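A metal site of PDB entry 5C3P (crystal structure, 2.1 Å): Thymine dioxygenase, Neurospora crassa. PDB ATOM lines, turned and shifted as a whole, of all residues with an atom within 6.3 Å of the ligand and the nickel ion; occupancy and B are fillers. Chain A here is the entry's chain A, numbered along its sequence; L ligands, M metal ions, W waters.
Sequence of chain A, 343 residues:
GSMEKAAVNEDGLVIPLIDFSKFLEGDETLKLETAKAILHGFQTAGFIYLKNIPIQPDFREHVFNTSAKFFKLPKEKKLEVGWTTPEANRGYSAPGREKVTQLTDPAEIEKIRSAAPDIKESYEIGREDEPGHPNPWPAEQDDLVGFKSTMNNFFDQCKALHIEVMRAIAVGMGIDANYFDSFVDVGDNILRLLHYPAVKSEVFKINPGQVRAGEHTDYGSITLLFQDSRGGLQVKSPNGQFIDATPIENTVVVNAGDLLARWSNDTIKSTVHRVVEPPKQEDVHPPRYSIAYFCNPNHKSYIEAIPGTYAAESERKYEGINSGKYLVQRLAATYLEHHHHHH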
ATOM      1  N   LYS A 120     -15.349   2.252  29.655  1.00  0.00           N
ATOM      2  CA  LYS A 120     -15.532   3.662  29.971  1.00  0.00           C
ATOM      3  C   LYS A 120     -15.870   3.856  31.427  1.00  0.00           C
ATOM      4  O   LYS A 120     -16.305   2.936  32.103  1.00  0.00           O
ATOM      5  CB  LYS A 120     -16.685   4.246  29.136  1.00  0.00           C
ATOM      6  CG  LYS A 120     -18.068   3.796  29.574  1.00  0.00           C
ATOM      7  CD  LYS A 120     -19.191   4.432  28.759  1.00  0.00           C
ATOM      8  CE  LYS A 120     -20.517   4.329  29.492  1.00  0.00           C
ATOM      9  NZ  LYS A 120     -21.671   4.771  28.653  1.00  0.00           N
ATOM     10  N   ARG A 192     -22.612  14.918  31.825  1.00  0.00           N
ATOM     11  CA  ARG A 192     -21.877  13.664  31.967  1.00  0.00           C
ATOM     12  C   ARG A 192     -20.451  13.762  31.431  1.00  0.00           C
ATOM     13  O   ARG A 192     -20.245  13.845  30.217  1.00  0.00           O
ATOM     14  CB  ARG A 192     -22.608  12.520  31.263  1.00  0.00           C
ATOM     15  CG  ARG A 192     -21.917  11.155  31.422  1.00  0.00           C
ATOM     16  CD  ARG A 192     -22.510  10.093  30.511  1.00  0.00           C
ATOM     17  NE  ARG A 192     -23.741   9.549  31.034  1.00  0.00           N
ATOM     18  CZ  ARG A 192     -24.534   8.691  30.391  1.00  0.00           C
ATOM     19  NH1 ARG A 192     -24.237   8.282  29.155  1.00  0.00           N
ATOM     20  NH2 ARG A 192     -25.641   8.265  30.973  1.00  0.00           N
ATOM     21  N   LEU A 194     -17.124  11.869  30.480  1.00  0.00           N
ATOM     22  CA  LEU A 194     -16.789  10.516  30.061  1.00  0.00           C
ATOM     23  C   LEU A 194     -15.298  10.351  29.860  1.00  0.00           C
ATOM     24  O   LEU A 194     -14.602  11.246  29.354  1.00  0.00           O
ATOM     25  CB  LEU A 194     -17.489  10.147  28.761  1.00  0.00           C
ATOM     26  CG  LEU A 194     -19.005   9.967  28.866  1.00  0.00           C
ATOM     27  CD1 LEU A 194     -19.722  10.381  27.595  1.00  0.00           C
ATOM     28  CD2 LEU A 194     -19.328   8.533  29.246  1.00  0.00           C
ATOM     29  N   TYR A 196     -12.805   7.260  28.364  1.00  0.00           N
ATOM     30  CA  TYR A 196     -12.565   5.935  27.824  1.00  0.00           C
ATOM     31  C   TYR A 196     -11.059   5.656  27.940  1.00  0.00           C
ATOM     32  O   TYR A 196     -10.253   6.278  27.238  1.00  0.00           O
ATOM     33  CB  TYR A 196     -13.033   5.870  26.370  1.00  0.00           C
ATOM     34  CG  TYR A 196     -14.491   6.275  26.145  1.00  0.00           C
ATOM     35  CD1 TYR A 196     -14.853   7.607  25.996  1.00  0.00           C
ATOM     36  CD2 TYR A 196     -15.492   5.304  26.056  1.00  0.00           C
ATOM     37  CE1 TYR A 196     -16.179   7.976  25.784  1.00  0.00           C
ATOM     38  CE2 TYR A 196     -16.821   5.662  25.818  1.00  0.00           C
ATOM     39  CZ  TYR A 196     -17.159   6.990  25.685  1.00  0.00           C
ATOM     40  OH  TYR A 196     -18.481   7.354  25.451  1.00  0.00           O
ATOM     41  N   ALA A 213     -18.545   2.537  23.647  1.00  0.00           N
ATOM     42  CA  ALA A 213     -19.900   2.787  24.118  1.00  0.00           C
ATOM     43  C   ALA A 213     -20.884   2.071  23.198  1.00  0.00           C
ATOM     44  O   ALA A 213     -20.855   2.259  21.967  1.00  0.00           O
ATOM     45  CB  ALA A 213     -20.217   4.271  24.146  1.00  0.00           C
ATOM     46  N   HIS A 216     -27.049   2.901  20.925  1.00  0.00           N
ATOM     47  CA  HIS A 216     -28.211   3.359  21.658  1.00  0.00           C
ATOM     48  C   HIS A 216     -28.733   4.627  21.021  1.00  0.00           C
ATOM     49  O   HIS A 216     -28.081   5.269  20.182  1.00  0.00           O
ATOM     50  CB  HIS A 216     -27.850   3.690  23.130  1.00  0.00           C
ATOM     51  CG  HIS A 216     -26.857   4.794  23.252  1.00  0.00           C
ATOM     52  ND1 HIS A 216     -25.516   4.614  22.976  1.00  0.00           N
ATOM     53  CD2 HIS A 216     -26.993   6.099  23.573  1.00  0.00           C
ATOM     54  CE1 HIS A 216     -24.879   5.757  23.142  1.00  0.00           C
ATOM     55  NE2 HIS A 216     -25.746   6.666  23.515  1.00  0.00           N
ATOM     56  N   THR A 217     -29.940   4.995  21.448  1.00  0.00           N
ATOM     57  CA  THR A 217     -30.441   6.344  21.257  1.00  0.00           C
ATOM     58  C   THR A 217     -30.500   7.011  22.618  1.00  0.00           C
ATOM     59  O   THR A 217     -30.706   6.339  23.628  1.00  0.00           O
ATOM     60  CB  THR A 217     -31.852   6.371  20.647  1.00  0.00           C
ATOM     61  OG1 THR A 217     -32.744   5.598  21.458  1.00  0.00           O
ATOM     62  CG2 THR A 217     -31.846   5.833  19.254  1.00  0.00           C
ATOM     63  N   ASP A 218     -30.310   8.323  22.650  1.00  0.00           N
ATOM     64  CA  ASP A 218     -30.470   9.082  23.875  1.00  0.00           C
ATOM     65  C   ASP A 218     -31.952   9.229  24.202  1.00  0.00           C
ATOM     66  O   ASP A 218     -32.796   9.240  23.293  1.00  0.00           O
ATOM     67  CB  ASP A 218     -29.822  10.471  23.730  1.00  0.00           C
ATOM     68  CG  ASP A 218     -28.313  10.414  23.579  1.00  0.00           C
ATOM     69  OD1 ASP A 218     -27.725   9.345  23.821  1.00  0.00           O
ATOM     70  OD2 ASP A 218     -27.697  11.438  23.239  1.00  0.00           O
ATOM     71  N   THR A 223     -29.036  16.398  23.151  1.00  0.00           N
ATOM     72  CA  THR A 223     -27.732  16.152  23.769  1.00  0.00           C
ATOM     73  C   THR A 223     -26.676  17.012  23.091  1.00  0.00           C
ATOM     74  O   THR A 223     -26.591  17.059  21.858  1.00  0.00           O
ATOM     75  CB  THR A 223     -27.320  14.666  23.672  1.00  0.00           C
ATOM     76  OG1 THR A 223     -28.290  13.878  24.324  1.00  0.00           O
ATOM     77  CG2 THR A 223     -25.964  14.413  24.313  1.00  0.00           C
ATOM     78  N   LEU A 225     -22.814  17.291  22.643  1.00  0.00           N
ATOM     79  CA  LEU A 225     -21.682  16.377  22.765  1.00  0.00           C
ATOM     80  C   LEU A 225     -20.376  17.052  22.378  1.00  0.00           C
ATOM     81  O   LEU A 225     -20.165  17.409  21.209  1.00  0.00           O
ATOM     82  CB  LEU A 225     -21.897  15.117  21.906  1.00  0.00           C
ATOM     83  CG  LEU A 225     -20.717  14.135  21.938  1.00  0.00           C
ATOM     84  CD1 LEU A 225     -20.589  13.463  23.310  1.00  0.00           C
ATOM     85  CD2 LEU A 225     -20.876  13.074  20.857  1.00  0.00           C
ATOM     86  N   PHE A 226     -19.496  17.187  23.373  1.00  0.00           N
ATOM     87  CA  PHE A 226     -18.169  17.736  23.175  1.00  0.00           C
ATOM     88  C   PHE A 226     -17.179  16.573  23.128  1.00  0.00           C
ATOM     89  O   PHE A 226     -17.057  15.831  24.087  1.00  0.00           O
ATOM     90  CB  PHE A 226     -17.834  18.667  24.333  1.00  0.00           C
ATOM     91  CG  PHE A 226     -18.811  19.795  24.520  1.00  0.00           C
ATOM     92  CD1 PHE A 226     -19.994  19.601  25.236  1.00  0.00           C
ATOM     93  CD2 PHE A 226     -18.558  21.049  23.995  1.00  0.00           C
ATOM     94  CE1 PHE A 226     -20.897  20.651  25.422  1.00  0.00           C
ATOM     95  CE2 PHE A 226     -19.455  22.099  24.172  1.00  0.00           C
ATOM     96  CZ  PHE A 226     -20.628  21.897  24.884  1.00  0.00           C
ATOM     97  N   GLN A 227     -16.494  16.402  22.007  1.00  0.00           N
ATOM     98  CA  GLN A 227     -15.516  15.315  21.918  1.00  0.00           C
ATOM     99  C   GLN A 227     -14.107  15.833  21.665  1.00  0.00           C
ATOM    100  O   GLN A 227     -13.924  16.879  21.054  1.00  0.00           O
ATOM    101  CB  GLN A 227     -15.937  14.292  20.857  1.00  0.00           C
ATOM    102  CG  GLN A 227     -16.055  14.846  19.430  1.00  0.00           C
ATOM    103  CD  GLN A 227     -16.308  13.754  18.394  1.00  0.00           C
ATOM    104  OE1 GLN A 227     -16.049  12.573  18.646  1.00  0.00           O
ATOM    105  NE2 GLN A 227     -16.790  14.151  17.228  1.00  0.00           N
ATOM    106  N   LEU A 233     -16.682   8.011  17.610  1.00  0.00           N
ATOM    107  CA  LEU A 233     -18.125   8.211  17.509  1.00  0.00           C
ATOM    108  C   LEU A 233     -18.644   7.824  16.123  1.00  0.00           C
ATOM    109  O   LEU A 233     -18.082   8.220  15.102  1.00  0.00           O
ATOM    110  CB  LEU A 233     -18.514   9.655  17.836  1.00  0.00           C
ATOM    111  CG  LEU A 233     -20.007   9.954  17.811  1.00  0.00           C
ATOM    112  CD1 LEU A 233     -20.741   9.240  18.917  1.00  0.00           C
ATOM    113  CD2 LEU A 233     -20.209  11.455  17.914  1.00  0.00           C
ATOM    114  N   ASN A 255     -27.424  16.220  19.028  1.00  0.00           N
ATOM    115  CA  ASN A 255     -28.391  15.237  18.543  1.00  0.00           C
ATOM    116  C   ASN A 255     -29.673  15.260  19.332  1.00  0.00           C
ATOM    117  O   ASN A 255     -29.685  15.582  20.513  1.00  0.00           O
ATOM    118  CB  ASN A 255     -27.815  13.839  18.555  1.00  0.00           C
ATOM    119  CG  ASN A 255     -27.597  13.307  19.940  1.00  0.00           C
ATOM    120  OD1 ASN A 255     -26.685  13.735  20.640  1.00  0.00           O
ATOM    121  ND2 ASN A 255     -28.427  12.326  20.357  1.00  0.00           N
ATOM    122  N   HIS A 273     -26.480   5.755  17.739  1.00  0.00           N
ATOM    123  CA  HIS A 273     -25.059   6.022  17.656  1.00  0.00           C
ATOM    124  C   HIS A 273     -24.314   5.203  18.698  1.00  0.00           C
ATOM    125  O   HIS A 273     -24.908   4.688  19.661  1.00  0.00           O
ATOM    126  CB  HIS A 273     -24.794   7.512  17.849  1.00  0.00           C
ATOM    127  CG  HIS A 273     -25.384   8.071  19.087  1.00  0.00           C
ATOM    128  ND1 HIS A 273     -26.750   8.219  19.262  1.00  0.00           N
ATOM    129  CD2 HIS A 273     -24.813   8.494  20.233  1.00  0.00           C
ATOM    130  CE1 HIS A 273     -26.982   8.717  20.459  1.00  0.00           C
ATOM    131  NE2 HIS A 273     -25.830   8.909  21.059  1.00  0.00           N
ATOM    132  N   ARG A 274     -23.000   5.132  18.515  1.00  0.00           N
ATOM    133  CA  ARG A 274     -22.109   4.345  19.366  1.00  0.00           C
ATOM    134  C   ARG A 274     -20.700   4.911  19.294  1.00  0.00           C
ATOM    135  O   ARG A 274     -20.409   5.779  18.475  1.00  0.00           O
ATOM    136  CB  ARG A 274     -22.090   2.856  18.905  1.00  0.00           C
ATOM    137  CG  ARG A 274     -21.447   2.660  17.541  1.00  0.00           C
ATOM    138  CD  ARG A 274     -21.513   1.212  17.037  1.00  0.00           C
ATOM    139  NE  ARG A 274     -20.702   1.064  15.832  1.00  0.00           N
ATOM    140  CZ  ARG A 274     -20.553  -0.062  15.153  1.00  0.00           C
ATOM    141  NH1 ARG A 274     -21.157  -1.164  15.559  1.00  0.00           N
ATOM    142  NH2 ARG A 274     -19.802  -0.084  14.042  1.00  0.00           N
ATOM    143  N   VAL A 275     -19.834   4.417  20.159  1.00  0.00           N
ATOM    144  CA  VAL A 275     -18.412   4.737  20.114  1.00  0.00           C
ATOM    145  C   VAL A 275     -17.622   3.450  19.994  1.00  0.00           C
ATOM    146  O   VAL A 275     -17.666   2.588  20.866  1.00  0.00           O
ATOM    147  CB  VAL A 275     -17.926   5.510  21.356  1.00  0.00           C
ATOM    148  CG1 VAL A 275     -16.472   5.932  21.167  1.00  0.00           C
ATOM    149  CG2 VAL A 275     -18.790   6.742  21.618  1.00  0.00           C
ATOM    150  N   ARG A 288      -9.571   8.529  25.556  1.00  0.00           N
ATOM    151  CA  ARG A 288     -10.491   9.427  24.868  1.00  0.00           C
ATOM    152  C   ARG A 288     -11.384  10.077  25.887  1.00  0.00           C
ATOM    153  O   ARG A 288     -11.929   9.395  26.735  1.00  0.00           O
ATOM    154  CB  ARG A 288     -11.343   8.679  23.843  1.00  0.00           C
ATOM    155  CG  ARG A 288     -12.528   9.470  23.289  1.00  0.00           C
ATOM    156  CD  ARG A 288     -13.153   8.742  22.102  1.00  0.00           C
ATOM    157  NE  ARG A 288     -14.128   9.594  21.424  1.00  0.00           N
ATOM    158  CZ  ARG A 288     -15.391   9.757  21.810  1.00  0.00           C
ATOM    159  NH1 ARG A 288     -15.874   9.143  22.879  1.00  0.00           N
ATOM    160  NH2 ARG A 288     -16.178  10.578  21.122  1.00  0.00           N
ATOM    161  N   TYR A 289     -11.518  11.395  25.804  1.00  0.00           N
ATOM    162  CA  TYR A 289     -12.421  12.154  26.640  1.00  0.00           C
ATOM    163  C   TYR A 289     -13.537  12.755  25.818  1.00  0.00           C
ATOM    164  O   TYR A 289     -13.303  13.268  24.715  1.00  0.00           O
ATOM    165  CB  TYR A 289     -11.679  13.291  27.339  1.00  0.00           C
ATOM    166  CG  TYR A 289     -10.625  12.786  28.279  1.00  0.00           C
ATOM    167  CD1 TYR A 289     -10.955  12.499  29.598  1.00  0.00           C
ATOM    168  CD2 TYR A 289      -9.329  12.566  27.854  1.00  0.00           C
ATOM    169  CE1 TYR A 289     -10.017  12.018  30.474  1.00  0.00           C
ATOM    170  CE2 TYR A 289      -8.373  12.084  28.730  1.00  0.00           C
ATOM    171  CZ  TYR A 289      -8.732  11.814  30.043  1.00  0.00           C
ATOM    172  OH  TYR A 289      -7.822  11.335  30.937  1.00  0.00           O
ATOM    173  N   SER A 290     -14.744  12.691  26.366  1.00  0.00           N
ATOM    174  CA  SER A 290     -15.883  13.414  25.817  1.00  0.00           C
ATOM    175  C   SER A 290     -16.735  13.883  26.979  1.00  0.00           C
ATOM    176  O   SER A 290     -16.565  13.448  28.120  1.00  0.00           O
ATOM    177  CB  SER A 290     -16.705  12.511  24.892  1.00  0.00           C
ATOM    178  OG  SER A 290     -17.310  11.481  25.633  1.00  0.00           O
ATOM    179  N   ILE A 291     -17.648  14.799  26.665  1.00  0.00           N
ATOM    180  CA  ILE A 291     -18.569  15.370  27.629  1.00  0.00           C
ATOM    181  C   ILE A 291     -19.927  15.491  26.948  1.00  0.00           C
ATOM    182  O   ILE A 291     -20.041  16.160  25.921  1.00  0.00           O
ATOM    183  CB  ILE A 291     -18.108  16.767  28.115  1.00  0.00           C
ATOM    184  CG1 ILE A 291     -16.758  16.658  28.838  1.00  0.00           C
ATOM    185  CG2 ILE A 291     -19.135  17.378  29.069  1.00  0.00           C
ATOM    186  CD1 ILE A 291     -16.140  18.000  29.186  1.00  0.00           C
ATOM    187  N   ALA A 292     -20.926  14.808  27.500  1.00  0.00           N
ATOM    188  CA  ALA A 292     -22.296  14.848  27.014  1.00  0.00           C
ATOM    189  C   ALA A 292     -23.173  15.621  27.998  1.00  0.00           C
ATOM    190  O   ALA A 292     -23.190  15.336  29.187  1.00  0.00           O
ATOM    191  CB  ALA A 292     -22.848  13.450  26.827  1.00  0.00           C
ATOM    192  N   PHE A 294     -26.921  16.197  28.658  1.00  0.00           N
ATOM    193  CA  PHE A 294     -28.238  15.686  28.313  1.00  0.00           C
ATOM    194  C   PHE A 294     -29.273  16.691  28.758  1.00  0.00           C
ATOM    195  O   PHE A 294     -29.411  16.957  29.976  1.00  0.00           O
ATOM    196  CB  PHE A 294     -28.484  14.328  28.972  1.00  0.00           C
ATOM    197  CG  PHE A 294     -27.505  13.269  28.549  1.00  0.00           C
ATOM    198  CD1 PHE A 294     -27.641  12.639  27.313  1.00  0.00           C
ATOM    199  CD2 PHE A 294     -26.460  12.903  29.379  1.00  0.00           C
ATOM    200  CE1 PHE A 294     -26.734  11.663  26.929  1.00  0.00           C
ATOM    201  CE2 PHE A 294     -25.558  11.926  29.003  1.00  0.00           C
ATOM    202  CZ  PHE A 294     -25.687  11.303  27.771  1.00  0.00           C
HETATM  203  C1  LIG L   1     -23.670   8.985  25.528  1.00  0.00           C
HETATM  204  O1  LIG L   1     -24.917   9.029  25.443  1.00  0.00           O
HETATM  205  O2  LIG L   1     -23.082   8.925  26.638  1.00  0.00           O
HETATM  206  C2  LIG L   1     -22.881   8.993  24.275  1.00  0.00           C
HETATM  207  O3  LIG L   1     -23.444   8.805  23.199  1.00  0.00           O
HETATM  208  C3  LIG L   1     -21.382   9.218  24.338  1.00  0.00           C
HETATM  209  C4  LIG L   1     -20.809   9.570  22.976  1.00  0.00           C
HETATM  210  C5  LIG L   1     -19.352   9.971  23.039  1.00  0.00           C
HETATM  211  O4  LIG L   1     -18.870  10.550  22.040  1.00  0.00           O
HETATM  212  O5  LIG L   1     -18.662   9.696  24.045  1.00  0.00           O
HETATM  213 NI    NI M   1     -25.594   8.981  23.281  1.00  0.00          NI
HETATM  214  O   HOH W   1     -26.732   7.799  26.992  1.00  0.00           O
HETATM  215  O   HOH W   2     -21.170   6.601  27.096  1.00  0.00           O
HETATM  216  O   HOH W   3     -25.152  11.234  23.199  1.00  0.00           O
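An oxygen (O5) of the ligand is in hydrogen-bond range of the side-chain hydroxyl of Tyr 196, at 2.7 Å.
The guanidinium group (NH2) of Arg 288 lies within salt-bridge range of an oxygen (O4) of the ligand (2.8 Å).
An oxygen (O5) of the ligand sits at hydrogen-bond distance from the side-chain hydroxyl (OG) of Ser 290, 2.7 Å away.
The guanidinium group (NH1) of Arg 192 is in salt-bridge range of an oxygen (O2) of the ligand, 2.8 Å away.
The backbone NH (N) of Tyr 196 sits at hydrogen-bond distance from the backbone carbonyl oxygen (O) of Arg 288 (2.8 Å).
OD2 of Asp 218 lies within hydrogen-bond range of ND2 of Asn 255 (3.1 Å).
The side-chain carboxylate (OD2) of Asp 218 sits at hydrogen-bond distance from the side-chain hydroxyl (OG1) of Thr 223 (2.7 Å).
The backbone carbonyl oxygen of Val 275 lies within hydrogen-bond range of the backbone NH of Ala 213.
The backbone NH of Arg 192 lies within hydrogen-bond range of the backbone carbonyl oxygen of Ala 292, 2.7 Å away.
The side-chain amide oxygen of Gln 227 is in hydrogen-bond range of the guanidinium group of Arg 288, 3.2 Å away.
O of Ser 290 sits at hydrogen-bond distance from N of Leu 194 (2.9 Å).
Leu 194 touches the ligand (CD1 to O5, 3.8 Å).
Leu 225 touches the ligand.
Leu 233 touches the ligand.
Val 275 touches the ligand (CG2 to C5, 3.6 Å).
Phe 294 touches the ligand (CZ to O1, 3.3 Å).
Hydrophobic or aromatic side chains within 4 Å of the ligand: Leu 194, Tyr 196, His 216, Leu 225, Leu 233, His 273, Val 275 and Phe 294.
Of the 23 residues printed, 12 come within 4 Å of the ligand.
Along chain A the residues within 4 Å of the ligand span positions 192 to 294.
The nearest printed residue that does not touch the ligand is Ala 292 (4.5 Å).
Three residues have an atom within 4 Å of the nickel ion: His 216, Asp 218 and His 273.
The nearest printed residue that does not touch the nickel ion is Phe 294 (4.7 Å).
The nickel ion is bound by an oxygen (O3) of the ligand (2.2 Å), the side-chain carboxylate of Asp 218 (2.2 Å), a ring nitrogen (NE2) of His 273 (2.2 Å), an oxygen (O1) of the ligand (2.3 Å), water W3 (2.3 Å) and a ring nitrogen (NE2) of His 216 (2.3 Å).
The nickel ion has six donor atoms within binding distance.
Water W2 lies within hydrogen-bond range of NZ of Lys 120 (2.5 Å), O2 of the ligand (3.0 Å) and OH of Tyr 196 (3.2 Å).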
